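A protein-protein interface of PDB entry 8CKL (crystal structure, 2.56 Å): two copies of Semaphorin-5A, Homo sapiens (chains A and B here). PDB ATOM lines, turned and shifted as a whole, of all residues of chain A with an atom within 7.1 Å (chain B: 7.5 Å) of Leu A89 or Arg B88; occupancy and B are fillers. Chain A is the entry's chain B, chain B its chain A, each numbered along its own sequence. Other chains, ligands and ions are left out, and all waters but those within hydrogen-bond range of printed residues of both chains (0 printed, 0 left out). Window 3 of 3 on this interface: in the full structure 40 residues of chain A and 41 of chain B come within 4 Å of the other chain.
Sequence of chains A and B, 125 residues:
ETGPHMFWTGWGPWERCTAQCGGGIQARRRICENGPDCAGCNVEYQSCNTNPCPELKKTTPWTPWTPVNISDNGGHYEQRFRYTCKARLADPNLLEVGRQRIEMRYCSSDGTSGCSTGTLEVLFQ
Lys A86 touches Leu B95, and with the chains exchanged Leu A95 touches Lys B86. Ala A87 touches Leu B94, and with the chains exchanged Leu A94 touches Ala B87. Arg A88 touches Leu B94, and with the chains exchanged Leu A94 touches Arg B88. Leu B89 touches its own counterpart, Leu A89. 13 positions are printed for both chains.
Of the printed residues of chain B, Ala A87 touches Leu B94 (3.3 Å) and Leu B95 (3.8 Å). Leu A89 touches just these residues of chain B: Arg B88 and Leu B89. Asn A93 touches none of the printed residues of chain B. Of the printed residues of chain B, Leu A95 touches Lys B86. Cys B21 touches none of the printed residues of chain A. Of the printed residues of chain A, Ala B87 touches Leu A94 (3.5 Å). Of the printed residues of chain A, Leu B95 touches Lys A86 (3.6 Å) and Ala A87 (3.8 Å). The nearest residue of chain B that does not touch Leu A89 is Ala B87 (4.2 Å). The nearest residue of chain A that does not touch Arg B88 is Leu A95 (5.6 Å).
Among the printed residues, merely in contact across the chains: Arg A88 with Leu B89 (3.3 Å), Ala A87 with Leu B94 (3.3 Å), Leu A89 with Arg B88 (3.3 Å), Leu A95 with Lys B86 (3.5 Å), Leu A94 with Ala B87 (3.5 Å), Leu A94 with Arg B88 (3.5 Å), Lys A86 with Leu B95 (3.6 Å), Leu A89 with Leu B89 (3.6 Å), Lys A86 with Leu B94 (3.7 Å), Ala A87 with Leu B95 (3.8 Å) and Leu A94 with Lys B86 (3.8 Å).
The backbone NH (N) of Leu A89 lies within hydrogen-bond range of the backbone carbonyl oxygen (O) of Pro A54. The backbone carbonyl oxygen (O) of Ala B87 is in hydrogen-bond range of the backbone NH (N) of Leu B56. The backbone NH of Leu B89 sits at hydrogen-bond distance from the backbone carbonyl oxygen of Pro B54 (3.4 Å). The backbone carbonyl oxygen (O) of Cys B53 sits at hydrogen-bond distance from the guanidinium group (NH1) of Arg B88 (3.0 Å). The side-chain carboxylate (OE2) of Glu B55 is in salt-bridge range of the side-chain amino group (NZ) of Lys B86 (3.9 Å). The side-chain sulfur (SG) of Cys B21 forms a disulfide with the side-chain sulfur (SG) of Cys B53 (2.0 Å).
Of the 14 printed residues of chain B, 6 touch a printed residue of chain A. Hydrophobic or aromatic side chains of chain B within 4 Å of the printed part of chain A: Leu B89 and Leu B95. Hydrophobic or aromatic side chains of chain A that line the printed part of chain B: Ala A87, Leu A89 and Leu A95. Among the printed residues, 13 pairs touch across the chains. Among the printed residues, no Asp or Glu carboxylate lies within 4 Å of a Lys or Arg side-chain nitrogen of the other chain.
N of Lys B86 is in hydrogen-bond range of O of Glu A96 (3.0 Å). The backbone carbonyl oxygen of Leu B94 sits at hydrogen-bond distance from the backbone NH of Arg A88, 3.4 Å away.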
ATOM      1  N   CYS A  21      10.349   0.155  12.507  1.00  0.00           N
ATOM      2  CA  CYS A  21      10.957  -0.732  11.525  1.00  0.00           C
ATOM      3  C   CYS A  21      12.339  -1.128  12.022  1.00  0.00           C
ATOM      4  O   CYS A  21      12.897  -0.503  12.929  1.00  0.00           O
ATOM      5  CB  CYS A  21      11.039  -0.076  10.141  1.00  0.00           C
ATOM      6  SG  CYS A  21      11.871   1.531  10.105  1.00  0.00           S
ATOM      7  N   CYS A  53      13.829  -0.963   7.277  1.00  0.00           N
ATOM      8  CA  CYS A  53      13.297   0.384   7.137  1.00  0.00           C
ATOM      9  C   CYS A  53      13.354   0.837   5.679  1.00  0.00           C
ATOM     10  O   CYS A  53      14.292   0.491   4.954  1.00  0.00           O
ATOM     11  CB  CYS A  53      14.079   1.355   8.018  1.00  0.00           C
ATOM     12  SG  CYS A  53      13.832   1.101   9.794  1.00  0.00           S
ATOM     13  N   PRO A  54      12.368   1.606   5.222  1.00  0.00           N
ATOM     14  CA  PRO A  54      12.371   2.079   3.836  1.00  0.00           C
ATOM     15  C   PRO A  54      13.434   3.141   3.596  1.00  0.00           C
ATOM     16  O   PRO A  54      13.925   3.796   4.517  1.00  0.00           O
ATOM     17  CB  PRO A  54      10.964   2.655   3.655  1.00  0.00           C
ATOM     18  CG  PRO A  54      10.567   3.080   5.028  1.00  0.00           C
ATOM     19  CD  PRO A  54      11.182   2.073   5.963  1.00  0.00           C
ATOM     20  N   GLU A  55      13.784   3.303   2.321  1.00  0.00           N
ATOM     21  CA  GLU A  55      14.764   4.300   1.903  1.00  0.00           C
ATOM     22  C   GLU A  55      14.027   5.593   1.572  1.00  0.00           C
ATOM     23  O   GLU A  55      13.245   5.647   0.618  1.00  0.00           O
ATOM     24  CB  GLU A  55      15.569   3.803   0.705  1.00  0.00           C
ATOM     25  N   LEU A  56      14.282   6.634   2.360  1.00  0.00           N
ATOM     26  CA  LEU A  56      13.661   7.936   2.184  1.00  0.00           C
ATOM     27  C   LEU A  56      14.507   8.797   1.258  1.00  0.00           C
ATOM     28  O   LEU A  56      15.736   8.855   1.390  1.00  0.00           O
ATOM     29  CB  LEU A  56      13.490   8.623   3.537  1.00  0.00           C
ATOM     30  CG  LEU A  56      12.897   7.727   4.626  1.00  0.00           C
ATOM     31  CD1 LEU A  56      12.836   8.455   5.954  1.00  0.00           C
ATOM     32  CD2 LEU A  56      11.519   7.232   4.221  1.00  0.00           C
ATOM     33  N   LYS A  86      19.380  10.140  -0.195  1.00  0.00           N
ATOM     34  CA  LYS A  86      18.716   8.882   0.117  1.00  0.00           C
ATOM     35  C   LYS A  86      19.272   8.347   1.427  1.00  0.00           C
ATOM     36  O   LYS A  86      20.492   8.315   1.618  1.00  0.00           O
ATOM     37  CB  LYS A  86      18.917   7.860  -1.005  1.00  0.00           C
ATOM     38  CG  LYS A  86      18.505   8.359  -2.381  1.00  0.00           C
ATOM     39  CD  LYS A  86      19.163   7.547  -3.482  1.00  0.00           C
ATOM     40  CE  LYS A  86      18.681   6.105  -3.468  1.00  0.00           C
ATOM     41  NZ  LYS A  86      19.294   5.302  -4.561  1.00  0.00           N
ATOM     42  N   ALA A  87      18.383   7.927   2.323  1.00  0.00           N
ATOM     43  CA  ALA A  87      18.822   7.431   3.621  1.00  0.00           C
ATOM     44  C   ALA A  87      17.819   6.424   4.161  1.00  0.00           C
ATOM     45  O   ALA A  87      16.611   6.597   4.002  1.00  0.00           O
ATOM     46  CB  ALA A  87      19.008   8.577   4.621  1.00  0.00           C
ATOM     47  N   ARG A  88      18.328   5.378   4.810  1.00  0.00           N
ATOM     48  CA  ARG A  88      17.479   4.348   5.407  1.00  0.00           C
ATOM     49  C   ARG A  88      17.079   4.820   6.799  1.00  0.00           C
ATOM     50  O   ARG A  88      17.858   4.723   7.750  1.00  0.00           O
ATOM     51  CB  ARG A  88      18.204   3.009   5.451  1.00  0.00           C
ATOM     52  N   LEU A  89      15.854   5.329   6.920  1.00  0.00           N
ATOM     53  CA  LEU A  89      15.363   5.898   8.164  1.00  0.00           C
ATOM     54  C   LEU A  89      13.893   5.548   8.343  1.00  0.00           C
ATOM     55  O   LEU A  89      13.206   5.149   7.400  1.00  0.00           O
ATOM     56  CB  LEU A  89      15.539   7.423   8.197  1.00  0.00           C
ATOM     57  CG  LEU A  89      16.949   7.976   8.391  1.00  0.00           C
ATOM     58  CD1 LEU A  89      17.043   9.386   7.834  1.00  0.00           C
ATOM     59  CD2 LEU A  89      17.307   7.961   9.865  1.00  0.00           C
ATOM     60  N   ALA A  90      13.420   5.703   9.579  1.00  0.00           N
ATOM     61  CA  ALA A  90      12.019   5.482   9.909  1.00  0.00           C
ATOM     62  C   ALA A  90      11.190   6.756   9.890  1.00  0.00           C
ATOM     63  O   ALA A  90       9.988   6.698   9.611  1.00  0.00           O
ATOM     64  CB  ALA A  90      11.895   4.833  11.291  1.00  0.00           C
ATOM     65  N   ASP A  91      11.803   7.902  10.180  1.00  0.00           N
ATOM     66  CA  ASP A  91      11.109   9.180  10.222  1.00  0.00           C
ATOM     67  C   ASP A  91      11.632  10.076   9.113  1.00  0.00           C
ATOM     68  O   ASP A  91      12.837  10.365   9.081  1.00  0.00           O
ATOM     69  CB  ASP A  91      11.302   9.845  11.586  1.00  0.00           C
ATOM     70  CG  ASP A  91      10.338  10.996  11.829  1.00  0.00           C
ATOM     71  OD1 ASP A  91       9.826  11.581  10.852  1.00  0.00           O
ATOM     72  OD2 ASP A  91      10.090  11.320  13.010  1.00  0.00           O
ATOM     73  N   PRO A  92      10.786  10.525   8.182  1.00  0.00           N
ATOM     74  CA  PRO A  92      11.267  11.450   7.142  1.00  0.00           C
ATOM     75  C   PRO A  92      11.791  12.759   7.702  1.00  0.00           C
ATOM     76  O   PRO A  92      12.613  13.411   7.047  1.00  0.00           O
ATOM     77  CB  PRO A  92      10.030  11.668   6.261  1.00  0.00           C
ATOM     78  CG  PRO A  92       8.870  11.326   7.141  1.00  0.00           C
ATOM     79  CD  PRO A  92       9.354  10.222   8.032  1.00  0.00           C
ATOM     80  N   ASN A  93      11.345  13.163   8.894  1.00  0.00           N
ATOM     81  CA  ASN A  93      11.834  14.396   9.497  1.00  0.00           C
ATOM     82  C   ASN A  93      13.292  14.291   9.925  1.00  0.00           C
ATOM     83  O   ASN A  93      13.925  15.321  10.176  1.00  0.00           O
ATOM     84  CB  ASN A  93      10.963  14.773  10.695  1.00  0.00           C
ATOM     85  CG  ASN A  93       9.514  15.004  10.313  1.00  0.00           C
ATOM     86  OD1 ASN A  93       9.209  15.347   9.170  1.00  0.00           O
ATOM     87  ND2 ASN A  93       8.611  14.815  11.268  1.00  0.00           N
ATOM     88  N   LEU A  94      13.836  13.076  10.015  1.00  0.00           N
ATOM     89  CA  LEU A  94      15.238  12.886  10.358  1.00  0.00           C
ATOM     90  C   LEU A  94      16.168  13.122   9.176  1.00  0.00           C
ATOM     91  O   LEU A  94      17.384  13.222   9.376  1.00  0.00           O
ATOM     92  CB  LEU A  94      15.461  11.477  10.912  1.00  0.00           C
ATOM     93  CG  LEU A  94      14.711  11.136  12.201  1.00  0.00           C
ATOM     94  CD1 LEU A  94      15.022   9.714  12.643  1.00  0.00           C
ATOM     95  CD2 LEU A  94      15.049  12.132  13.301  1.00  0.00           C
ATOM     96  N   LEU A  95      15.631  13.206   7.964  1.00  0.00           N
ATOM     97  CA  LEU A  95      16.405  13.487   6.763  1.00  0.00           C
ATOM     98  C   LEU A  95      16.120  14.914   6.319  1.00  0.00           C
ATOM     99  O   LEU A  95      14.956  15.312   6.206  1.00  0.00           O
ATOM    100  CB  LEU A  95      16.061  12.502   5.644  1.00  0.00           C
ATOM    101  CG  LEU A  95      16.743  12.735   4.294  1.00  0.00           C
ATOM    102  CD1 LEU A  95      18.255  12.654   4.433  1.00  0.00           C
ATOM    103  CD2 LEU A  95      16.242  11.742   3.258  1.00  0.00           C
ATOM    104  N   GLU A  96      17.179  15.684   6.082  1.00  0.00           N
ATOM    105  CA  GLU A  96      17.038  17.077   5.691  1.00  0.00           C
ATOM    106  C   GLU A  96      18.116  17.430   4.677  1.00  0.00           C
ATOM    107  O   GLU A  96      19.174  16.800   4.616  1.00  0.00           O
ATOM    108  CB  GLU A  96      17.119  18.015   6.904  1.00  0.00           C
ATOM    109  N   CYS B  21      22.745   3.918  18.919  1.00  0.00           N
ATOM    110  CA  CYS B  21      22.213   5.204  19.340  1.00  0.00           C
ATOM    111  C   CYS B  21      20.745   5.273  18.948  1.00  0.00           C
ATOM    112  O   CYS B  21      20.264   4.482  18.132  1.00  0.00           O
ATOM    113  CB  CYS B  21      22.987   6.362  18.706  1.00  0.00           C
ATOM    114  SG  CYS B  21      23.048   6.269  16.901  1.00  0.00           S
ATOM    115  N   PRO B  52      21.079  10.533  21.515  1.00  0.00           N
ATOM    116  CA  PRO B  52      20.664  10.740  20.124  1.00  0.00           C
ATOM    117  C   PRO B  52      21.795  10.447  19.150  1.00  0.00           C
ATOM    118  O   PRO B  52      22.971  10.686  19.436  1.00  0.00           O
ATOM    119  CB  PRO B  52      20.263  12.220  20.088  1.00  0.00           C
ATOM    120  CG  PRO B  52      21.019  12.840  21.217  1.00  0.00           C
ATOM    121  CD  PRO B  52      21.083  11.788  22.285  1.00  0.00           C
ATOM    122  N   CYS B  53      21.423   9.915  17.989  1.00  0.00           N
ATOM    123  CA  CYS B  53      22.407   9.577  16.977  1.00  0.00           C
ATOM    124  C   CYS B  53      23.056  10.840  16.417  1.00  0.00           C
ATOM    125  O   CYS B  53      22.411  11.888  16.317  1.00  0.00           O
ATOM    126  CB  CYS B  53      21.772   8.782  15.843  1.00  0.00           C
ATOM    127  SG  CYS B  53      21.299   7.108  16.293  1.00  0.00           S
ATOM    128  N   PRO B  54      24.331  10.768  16.048  1.00  0.00           N
ATOM    129  CA  PRO B  54      24.997  11.946  15.490  1.00  0.00           C
ATOM    130  C   PRO B  54      24.435  12.280  14.120  1.00  0.00           C
ATOM    131  O   PRO B  54      23.870  11.434  13.423  1.00  0.00           O
ATOM    132  CB  PRO B  54      26.468  11.520  15.397  1.00  0.00           C
ATOM    133  CG  PRO B  54      26.587  10.308  16.275  1.00  0.00           C
ATOM    134  CD  PRO B  54      25.256   9.635  16.207  1.00  0.00           C
ATOM    135  N   GLU B  55      24.597  13.542  13.738  1.00  0.00           N
ATOM    136  CA  GLU B  55      24.116  14.018  12.447  1.00  0.00           C
ATOM    137  C   GLU B  55      25.232  13.876  11.421  1.00  0.00           C
ATOM    138  O   GLU B  55      26.268  14.542  11.520  1.00  0.00           O
ATOM    139  CB  GLU B  55      23.635  15.462  12.547  1.00  0.00           C
ATOM    140  CG  GLU B  55      23.008  15.984  11.266  1.00  0.00           C
ATOM    141  CD  GLU B  55      21.940  17.024  11.525  1.00  0.00           C
ATOM    142  OE1 GLU B  55      21.784  17.439  12.693  1.00  0.00           O
ATOM    143  OE2 GLU B  55      21.251  17.420  10.562  1.00  0.00           O
ATOM    144  N   LEU B  56      25.020  13.007  10.437  1.00  0.00           N
ATOM    145  CA  LEU B  56      25.976  12.783   9.370  1.00  0.00           C
ATOM    146  C   LEU B  56      25.668  13.742   8.232  1.00  0.00           C
ATOM    147  O   LEU B  56      24.504  13.893   7.836  1.00  0.00           O
ATOM    148  CB  LEU B  56      25.905  11.337   8.880  1.00  0.00           C
ATOM    149  CG  LEU B  56      25.879  10.264   9.970  1.00  0.00           C
ATOM    150  CD1 LEU B  56      25.719   8.884   9.359  1.00  0.00           C
ATOM    151  CD2 LEU B  56      27.133  10.329  10.823  1.00  0.00           C
ATOM    152  N   LYS B  86      21.885  15.830   5.297  1.00  0.00           N
ATOM    153  CA  LYS B  86      22.010  15.682   6.739  1.00  0.00           C
ATOM    154  C   LYS B  86      21.052  14.596   7.201  1.00  0.00           C
ATOM    155  O   LYS B  86      19.875  14.606   6.830  1.00  0.00           O
ATOM    156  CB  LYS B  86      21.693  17.002   7.447  1.00  0.00           C
ATOM    157  CG  LYS B  86      22.504  18.183   6.942  1.00  0.00           C
ATOM    158  CD  LYS B  86      21.818  19.504   7.257  1.00  0.00           C
ATOM    159  CE  LYS B  86      21.729  19.753   8.750  1.00  0.00           C
ATOM    160  NZ  LYS B  86      21.084  21.062   9.048  1.00  0.00           N
ATOM    161  N   ALA B  87      21.554  13.663   8.005  1.00  0.00           N
ATOM    162  CA  ALA B  87      20.706  12.579   8.485  1.00  0.00           C
ATOM    163  C   ALA B  87      21.225  12.064   9.817  1.00  0.00           C
ATOM    164  O   ALA B  87      22.433  11.928  10.005  1.00  0.00           O
ATOM    165  CB  ALA B  87      20.642  11.433   7.468  1.00  0.00           C
ATOM    166  N   ARG B  88      20.308  11.761  10.733  1.00  0.00           N
ATOM    167  CA  ARG B  88      20.679  11.211  12.036  1.00  0.00           C
ATOM    168  C   ARG B  88      20.759   9.696  11.898  1.00  0.00           C
ATOM    169  O   ARG B  88      19.738   9.003  11.901  1.00  0.00           O
ATOM    170  CB  ARG B  88      19.688  11.641  13.110  1.00  0.00           C
ATOM    171  CG  ARG B  88      19.711  13.138  13.377  1.00  0.00           C
ATOM    172  CD  ARG B  88      19.125  13.488  14.734  1.00  0.00           C
ATOM    173  NE  ARG B  88      19.288  14.905  15.037  1.00  0.00           N
ATOM    174  CZ  ARG B  88      20.382  15.434  15.568  1.00  0.00           C
ATOM    175  NH1 ARG B  88      21.433  14.690  15.874  1.00  0.00           N
ATOM    176  NH2 ARG B  88      20.426  16.744  15.794  1.00  0.00           N
ATOM    177  N   LEU B  89      21.981   9.179  11.779  1.00  0.00           N
ATOM    178  CA  LEU B  89      22.208   7.760  11.551  1.00  0.00           C
ATOM    179  C   LEU B  89      23.440   7.308  12.319  1.00  0.00           C
ATOM    180  O   LEU B  89      24.264   8.118  12.751  1.00  0.00           O
ATOM    181  CB  LEU B  89      22.390   7.451  10.058  1.00  0.00           C
ATOM    182  CG  LEU B  89      21.151   7.498   9.166  1.00  0.00           C
ATOM    183  CD1 LEU B  89      21.548   7.751   7.722  1.00  0.00           C
ATOM    184  CD2 LEU B  89      20.383   6.195   9.286  1.00  0.00           C
ATOM    185  N   ALA B  90      23.554   5.991  12.484  1.00  0.00           N
ATOM    186  CA  ALA B  90      24.712   5.384  13.128  1.00  0.00           C
ATOM    187  C   ALA B  90      25.769   4.919  12.138  1.00  0.00           C
ATOM    188  O   ALA B  90      26.956   4.899  12.480  1.00  0.00           O
ATOM    189  CB  ALA B  90      24.278   4.196  13.993  1.00  0.00           C
ATOM    190  N   ASP B  91      25.367   4.548  10.923  1.00  0.00           N
ATOM    191  CA  ASP B  91      26.286   4.065   9.902  1.00  0.00           C
ATOM    192  C   ASP B  91      26.329   5.063   8.756  1.00  0.00           C
ATOM    193  O   ASP B  91      25.285   5.331   8.140  1.00  0.00           O
ATOM    194  CB  ASP B  91      25.855   2.686   9.398  1.00  0.00           C
ATOM    195  CG  ASP B  91      26.944   1.977   8.609  1.00  0.00           C
ATOM    196  OD1 ASP B  91      27.845   2.654   8.070  1.00  0.00           O
ATOM    197  OD2 ASP B  91      26.898   0.732   8.525  1.00  0.00           O
ATOM    198  N   LEU B  94      24.689   4.256   5.310  1.00  0.00           N
ATOM    199  CA  LEU B  94      23.246   4.313   5.119  1.00  0.00           C
ATOM    200  C   LEU B  94      22.785   5.618   4.487  1.00  0.00           C
ATOM    201  O   LEU B  94      21.632   5.702   4.052  1.00  0.00           O
ATOM    202  CB  LEU B  94      22.530   4.109   6.456  1.00  0.00           C
ATOM    203  CG  LEU B  94      22.768   2.764   7.142  1.00  0.00           C
ATOM    204  CD1 LEU B  94      22.002   2.688   8.455  1.00  0.00           C
ATOM    205  CD2 LEU B  94      22.381   1.616   6.221  1.00  0.00           C
ATOM    206  N   LEU B  95      23.647   6.629   4.427  1.00  0.00           N
ATOM    207  CA  LEU B  95      23.339   7.902   3.792  1.00  0.00           C
ATOM    208  C   LEU B  95      24.100   7.995   2.478  1.00  0.00           C
ATOM    209  O   LEU B  95      25.315   7.777   2.444  1.00  0.00           O
ATOM    210  CB  LEU B  95      23.708   9.075   4.704  1.00  0.00           C
ATOM    211  CG  LEU B  95      23.511  10.473   4.118  1.00  0.00           C
ATOM    212  CD1 LEU B  95      22.055  10.696   3.745  1.00  0.00           C
ATOM    213  CD2 LEU B  95      23.983  11.533   5.099  1.00  0.00           C
